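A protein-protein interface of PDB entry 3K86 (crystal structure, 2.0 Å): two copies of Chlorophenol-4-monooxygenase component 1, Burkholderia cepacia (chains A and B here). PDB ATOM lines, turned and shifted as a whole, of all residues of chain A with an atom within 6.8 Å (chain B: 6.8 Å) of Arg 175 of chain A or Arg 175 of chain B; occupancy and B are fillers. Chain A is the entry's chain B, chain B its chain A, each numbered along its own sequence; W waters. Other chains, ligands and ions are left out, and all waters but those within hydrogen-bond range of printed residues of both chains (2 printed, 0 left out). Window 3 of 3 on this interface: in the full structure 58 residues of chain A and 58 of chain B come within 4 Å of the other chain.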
ATOM      1  N   ALA A  89      -0.667 -14.958   4.313  1.00  0.00           N
ATOM      2  CA  ALA A  89       0.400 -14.489   5.199  1.00  0.00           C
ATOM      3  C   ALA A  89       1.162 -15.621   5.860  1.00  0.00           C
ATOM      4  O   ALA A  89       2.368 -15.496   6.040  1.00  0.00           O
ATOM      5  CB  ALA A  89      -0.136 -13.539   6.257  1.00  0.00           C
ATOM      6  N   THR A 162      -5.536 -12.847   4.492  1.00  0.00           N
ATOM      7  CA  THR A 162      -4.505 -11.835   4.526  1.00  0.00           C
ATOM      8  C   THR A 162      -3.327 -12.245   3.639  1.00  0.00           C
ATOM      9  O   THR A 162      -2.903 -13.387   3.618  1.00  0.00           O
ATOM     10  CB  THR A 162      -4.036 -11.643   5.945  1.00  0.00           C
ATOM     11  OG1 THR A 162      -3.852 -12.934   6.520  1.00  0.00           O
ATOM     12  CG2 THR A 162      -5.108 -10.914   6.738  1.00  0.00           C
ATOM     13  N   TYR A 171       9.513 -10.738   3.219  1.00  0.00           N
ATOM     14  CA  TYR A 171       8.080 -11.018   3.275  1.00  0.00           C
ATOM     15  C   TYR A 171       7.351 -10.044   4.188  1.00  0.00           C
ATOM     16  O   TYR A 171       7.917  -9.532   5.154  1.00  0.00           O
ATOM     17  CB  TYR A 171       7.875 -12.427   3.772  1.00  0.00           C
ATOM     18  CG  TYR A 171       8.360 -13.458   2.799  1.00  0.00           C
ATOM     19  CD1 TYR A 171       7.735 -13.613   1.541  1.00  0.00           C
ATOM     20  CD2 TYR A 171       9.424 -14.299   3.128  1.00  0.00           C
ATOM     21  CE1 TYR A 171       8.169 -14.572   0.652  1.00  0.00           C
ATOM     22  CE2 TYR A 171       9.856 -15.257   2.257  1.00  0.00           C
ATOM     23  CZ  TYR A 171       9.219 -15.391   1.013  1.00  0.00           C
ATOM     24  OH  TYR A 171       9.662 -16.343   0.137  1.00  0.00           O
ATOM     25  N   ALA A 172       6.090  -9.797   3.896  1.00  0.00           N
ATOM     26  CA  ALA A 172       5.287  -8.924   4.738  1.00  0.00           C
ATOM     27  C   ALA A 172       3.861  -9.308   4.560  1.00  0.00           C
ATOM     28  O   ALA A 172       3.523 -10.074   3.647  1.00  0.00           O
ATOM     29  CB  ALA A 172       5.471  -7.451   4.338  1.00  0.00           C
ATOM     30  N   THR A 173       3.007  -8.729   5.388  1.00  0.00           N
ATOM     31  CA  THR A 173       1.597  -8.865   5.196  1.00  0.00           C
ATOM     32  C   THR A 173       1.035  -7.493   5.372  1.00  0.00           C
ATOM     33  O   THR A 173       1.806  -6.546   5.485  1.00  0.00           O
ATOM     34  CB  THR A 173       0.946  -9.894   6.116  1.00  0.00           C
ATOM     35  OG1 THR A 173      -0.413 -10.092   5.680  1.00  0.00           O
ATOM     36  CG2 THR A 173       0.970  -9.411   7.607  1.00  0.00           C
ATOM     37  N   THR A 174      -0.291  -7.364   5.326  1.00  0.00           N
ATOM     38  CA  THR A 174      -0.923  -6.055   5.347  1.00  0.00           C
ATOM     39  C   THR A 174      -1.345  -5.621   6.747  1.00  0.00           C
ATOM     40  O   THR A 174      -1.681  -6.445   7.582  1.00  0.00           O
ATOM     41  CB  THR A 174      -2.185  -6.043   4.514  1.00  0.00           C
ATOM     42  OG1 THR A 174      -3.018  -7.116   4.951  1.00  0.00           O
ATOM     43  CG2 THR A 174      -1.856  -6.233   3.012  1.00  0.00           C
ATOM     44  N   ARG A 175      -1.343  -4.316   6.979  1.00  0.00           N
ATOM     45  CA  ARG A 175      -2.056  -3.718   8.119  1.00  0.00           C
ATOM     46  C   ARG A 175      -2.900  -2.548   7.615  1.00  0.00           C
ATOM     47  O   ARG A 175      -2.688  -2.076   6.507  1.00  0.00           O
ATOM     48  CB  ARG A 175      -1.077  -3.242   9.198  1.00  0.00           C
ATOM     49  CG  ARG A 175      -0.178  -2.113   8.768  1.00  0.00           C
ATOM     50  CD  ARG A 175       0.507  -1.517   9.970  1.00  0.00           C
ATOM     51  NE  ARG A 175       1.658  -0.695   9.606  1.00  0.00           N
ATOM     52  CZ  ARG A 175       1.581   0.608   9.329  1.00  0.00           C
ATOM     53  NH1 ARG A 175       2.681   1.283   8.996  1.00  0.00           N
ATOM     54  NH2 ARG A 175       0.403   1.238   9.368  1.00  0.00           N
ATOM     55  N   SER A 176      -3.871  -2.085   8.396  1.00  0.00           N
ATOM     56  CA  SER A 176      -4.658  -0.942   7.945  1.00  0.00           C
ATOM     57  C   SER A 176      -3.841   0.335   8.056  1.00  0.00           C
ATOM     58  O   SER A 176      -2.811   0.378   8.750  1.00  0.00           O
ATOM     59  CB  SER A 176      -5.981  -0.832   8.688  1.00  0.00           C
ATOM     60  OG  SER A 176      -5.781  -1.010  10.069  1.00  0.00           O
ATOM     61  N   LEU A 177      -4.288   1.369   7.342  1.00  0.00           N
ATOM     62  CA  LEU A 177      -3.511   2.603   7.227  1.00  0.00           C
ATOM     63  C   LEU A 177      -3.300   3.352   8.557  1.00  0.00           C
ATOM     64  O   LEU A 177      -4.244   3.878   9.144  1.00  0.00           O
ATOM     65  CB  LEU A 177      -4.128   3.515   6.170  1.00  0.00           C
ATOM     66  CG  LEU A 177      -3.881   2.948   4.765  1.00  0.00           C
ATOM     67  CD1 LEU A 177      -4.248   3.937   3.683  1.00  0.00           C
ATOM     68  CD2 LEU A 177      -2.401   2.567   4.679  1.00  0.00           C
ATOM     69  N   ALA B  89       2.407   4.605   1.382  1.00  0.00           N
ATOM     70  CA  ALA B  89       1.313   4.451   2.340  1.00  0.00           C
ATOM     71  C   ALA B  89       0.519   5.720   2.614  1.00  0.00           C
ATOM     72  O   ALA B  89      -0.699   5.669   2.813  1.00  0.00           O
ATOM     73  CB  ALA B  89       1.837   3.861   3.684  1.00  0.00           C
ATOM     74  N   THR B 162       6.645   2.940   3.266  1.00  0.00           N
ATOM     75  CA  THR B 162       6.029   1.687   2.950  1.00  0.00           C
ATOM     76  C   THR B 162       5.009   1.842   1.786  1.00  0.00           C
ATOM     77  O   THR B 162       4.639   2.958   1.427  1.00  0.00           O
ATOM     78  CB  THR B 162       5.415   1.066   4.201  1.00  0.00           C
ATOM     79  OG1 THR B 162       4.389   1.930   4.722  1.00  0.00           O
ATOM     80  CG2 THR B 162       6.499   0.821   5.262  1.00  0.00           C
ATOM     81  N   TYR B 171      -7.713   0.228   1.250  1.00  0.00           N
ATOM     82  CA  TYR B 171      -6.284   0.529   1.239  1.00  0.00           C
ATOM     83  C   TYR B 171      -5.663  -0.047   2.491  1.00  0.00           C
ATOM     84  O   TYR B 171      -6.327  -0.162   3.500  1.00  0.00           O
ATOM     85  CB  TYR B 171      -6.074   2.047   1.254  1.00  0.00           C
ATOM     86  CG  TYR B 171      -6.566   2.734  -0.008  1.00  0.00           C
ATOM     87  CD1 TYR B 171      -5.881   2.555  -1.211  1.00  0.00           C
ATOM     88  CD2 TYR B 171      -7.698   3.536  -0.012  1.00  0.00           C
ATOM     89  CE1 TYR B 171      -6.298   3.148  -2.385  1.00  0.00           C
ATOM     90  CE2 TYR B 171      -8.151   4.134  -1.220  1.00  0.00           C
ATOM     91  CZ  TYR B 171      -7.430   3.930  -2.391  1.00  0.00           C
ATOM     92  OH  TYR B 171      -7.803   4.474  -3.594  1.00  0.00           O
ATOM     93  N   ALA B 172      -4.373  -0.349   2.424  1.00  0.00           N
ATOM     94  CA  ALA B 172      -3.629  -0.935   3.509  1.00  0.00           C
ATOM     95  C   ALA B 172      -2.180  -0.613   3.242  1.00  0.00           C
ATOM     96  O   ALA B 172      -1.843  -0.112   2.168  1.00  0.00           O
ATOM     97  CB  ALA B 172      -3.823  -2.428   3.509  1.00  0.00           C
ATOM     98  N   THR B 173      -1.310  -0.916   4.204  1.00  0.00           N
ATOM     99  CA  THR B 173       0.120  -0.912   3.951  1.00  0.00           C
ATOM    100  C   THR B 173       0.713  -2.178   4.545  1.00  0.00           C
ATOM    101  O   THR B 173      -0.023  -3.082   4.935  1.00  0.00           O
ATOM    102  CB  THR B 173       0.791   0.397   4.429  1.00  0.00           C
ATOM    103  OG1 THR B 173       2.179   0.384   4.055  1.00  0.00           O
ATOM    104  CG2 THR B 173       0.618   0.597   5.983  1.00  0.00           C
ATOM    105  N   THR B 174       2.031  -2.278   4.588  1.00  0.00           N
ATOM    106  CA  THR B 174       2.647  -3.525   5.000  1.00  0.00           C
ATOM    107  C   THR B 174       3.078  -3.539   6.474  1.00  0.00           C
ATOM    108  O   THR B 174       3.255  -2.497   7.084  1.00  0.00           O
ATOM    109  CB  THR B 174       3.888  -3.831   4.167  1.00  0.00           C
ATOM    110  OG1 THR B 174       4.746  -2.688   4.150  1.00  0.00           O
ATOM    111  CG2 THR B 174       3.470  -4.240   2.728  1.00  0.00           C
ATOM    112  N   ARG B 175       3.242  -4.734   7.008  1.00  0.00           N
ATOM    113  CA  ARG B 175       3.936  -4.975   8.287  1.00  0.00           C
ATOM    114  C   ARG B 175       4.681  -6.296   8.166  1.00  0.00           C
ATOM    115  O   ARG B 175       4.321  -7.155   7.336  1.00  0.00           O
ATOM    116  CB  ARG B 175       2.944  -5.099   9.433  1.00  0.00           C
ATOM    117  CG  ARG B 175       1.687  -5.856   9.081  1.00  0.00           C
ATOM    118  CD  ARG B 175       0.945  -6.332  10.323  1.00  0.00           C
ATOM    119  NE  ARG B 175       1.531  -7.574  10.797  1.00  0.00           N
ATOM    120  CZ  ARG B 175       0.840  -8.685  11.024  1.00  0.00           C
ATOM    121  NH1 ARG B 175       1.469  -9.786  11.425  1.00  0.00           N
ATOM    122  NH2 ARG B 175      -0.477  -8.693  10.856  1.00  0.00           N
ATOM    123  N   SER B 176       5.702  -6.484   9.000  1.00  0.00           N
ATOM    124  CA  SER B 176       6.459  -7.743   9.002  1.00  0.00           C
ATOM    125  C   SER B 176       5.568  -8.892   9.479  1.00  0.00           C
ATOM    126  O   SER B 176       4.532  -8.669  10.141  1.00  0.00           O
ATOM    127  CB  SER B 176       7.676  -7.604   9.902  1.00  0.00           C
ATOM    128  OG  SER B 176       7.263  -7.145  11.175  1.00  0.00           O
ATOM    129  N   LEU B 177       5.948 -10.124   9.136  1.00  0.00           N
ATOM    130  CA  LEU B 177       5.066 -11.271   9.372  1.00  0.00           C
ATOM    131  C   LEU B 177       4.680 -11.552  10.849  1.00  0.00           C
ATOM    132  O   LEU B 177       5.536 -11.626  11.732  1.00  0.00           O
ATOM    133  CB  LEU B 177       5.645 -12.504   8.710  1.00  0.00           C
ATOM    134  CG  LEU B 177       5.591 -12.375   7.185  1.00  0.00           C
ATOM    135  CD1 LEU B 177       5.800 -13.716   6.577  1.00  0.00           C
ATOM    136  CD2 LEU B 177       4.251 -11.843   6.771  1.00  0.00           C
HETATM  137  O   HOH W   1      -6.805   1.122   6.022  1.00  0.00           O
HETATM  138  O   HOH W   2       8.383 -10.336   7.788  1.00  0.00           O
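Of the 9 printed residues of chain A, 7 touch a printed residue of chain B.
Hydrophobic or aromatic side chains of chain A that line the printed part of chain B: Tyr 171, Ala 172 and Leu 177.
Along chain A the printed residues that touch a printed residue of chain B span positions 89 to 177.
Of the 9 printed residues of chain B, 6 touch a printed residue of chain A.
Printed residues of chain B that touch a printed residue of chain A: Tyr 171, Ala 172, Thr 173, Thr 174, Arg 175 and Leu 177.
Hydrophobic or aromatic side chains of chain B that line the printed part of chain A: Tyr 171, Ala 172 and Leu 177.
Among the printed residues, 18 pairs touch across the chains.
Among the printed residues, no Asp or Glu carboxylate lies within 4 Å of a Lys or Arg side-chain nitrogen of the other chain.
Tyr 171 of chain A touches Leu 177 of chain B, and with the chains exchanged Leu 177 of chain A touches Tyr 171 of chain B.
Ala 172 of chain A touches Leu 177 of chain B, and with the chains exchanged Leu 177 of chain A touches Ala 172 of chain B.
Thr 173 of chain B touches its own counterpart, Thr 173 of chain A.
Thr 174 of chain A touches Arg 175 of chain B, and with the chains exchanged Arg 175 of chain A touches Thr 174 of chain B.
Positions printed for both chains: 89, 162, 171, 172, 173, 174, 175, 176 and 177.
Of the 18 pairs that touch across the chains among the printed residues, 16 have their exchanged pair printed and touching as well.
OG1 of Thr 162 of chain B sits at hydrogen-bond distance from OG1 of Thr 173 of chain B (2.8 Å).
N of Ala 89 of chain A sits at hydrogen-bond distance from O of Thr 162 of chain A.
The backbone carbonyl oxygen (O) of Thr 173 of chain A is in hydrogen-bond range of the backbone NH (N) of Arg 175 of chain B, 2.8 Å away.
NE of Arg 175 of chain A is in hydrogen-bond range of O of Thr 174 of chain B, 3.5 Å away.
O of Thr 173 of chain B is in hydrogen-bond range of N of Arg 175 of chain A (2.7 Å).
Of the printed residues of chain B, Ala 89 of chain A touches Leu 177 (3.9 Å).
Thr 162 of chain A touches none of the printed residues of chain B.
Of the printed residues of chain B, Tyr 171 of chain A touches Leu 177.
Of the printed residues of chain B, Thr 174 of chain A touches Thr 173 (3.1 Å) and Arg 175 (3.7 Å).
Arg 175 of chain A touches just these residues of chain B: Ala 172, Thr 173, Thr 174 and Arg 175.
Ala 89 of chain B touches none of the printed residues of chain A.
Of the printed residues of chain A, Ala 172 of chain B touches Arg 175 and Leu 177.
The nearest residue of chain B that does not touch Arg 175 of chain A is Thr 162 of chain B (4.6 Å).
The nearest residue of chain A that does not touch Arg 175 of chain B is Tyr 171 of chain A (4.8 Å).
Among the printed residues, pairs that only touch across the chains: Ala 89 of chain A with Leu 177 of chain B, Tyr 171 of chain A with Leu 177 of chain B, Ala 172 of chain A with Thr 174 of chain B, Ala 172 of chain A with Arg 175 of chain B, Ala 172 of chain A with Leu 177 of chain B, Thr 173 of chain A with Thr 173 of chain B, Thr 173 of chain A with Thr 174 of chain B, Thr 173 of chain A with Leu 177 of chain B, Thr 174 of chain A with Thr 173 of chain B, Thr 174 of chain A with Arg 175 of chain B, Arg 175 of chain A with Ala 172 of chain B, Arg 175 of chain A with Arg 175 of chain B, Leu 177 of chain A with Tyr 171 of chain B, Leu 177 of chain A with Ala 172 of chain B and Leu 177 of chain A with Thr 173 of chain B.
Water W2 bridges the backbone NH (N) of Leu 177 of chain B (2.8 Å) and the backbone carbonyl oxygen (O) of Tyr 171 of chain A (2.8 Å).
Water W1 bridges the backbone NH (N) of Leu 177 of chain A (2.9 Å) and the backbone carbonyl oxygen (O) of Tyr 171 of chain B (2.9 Å).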
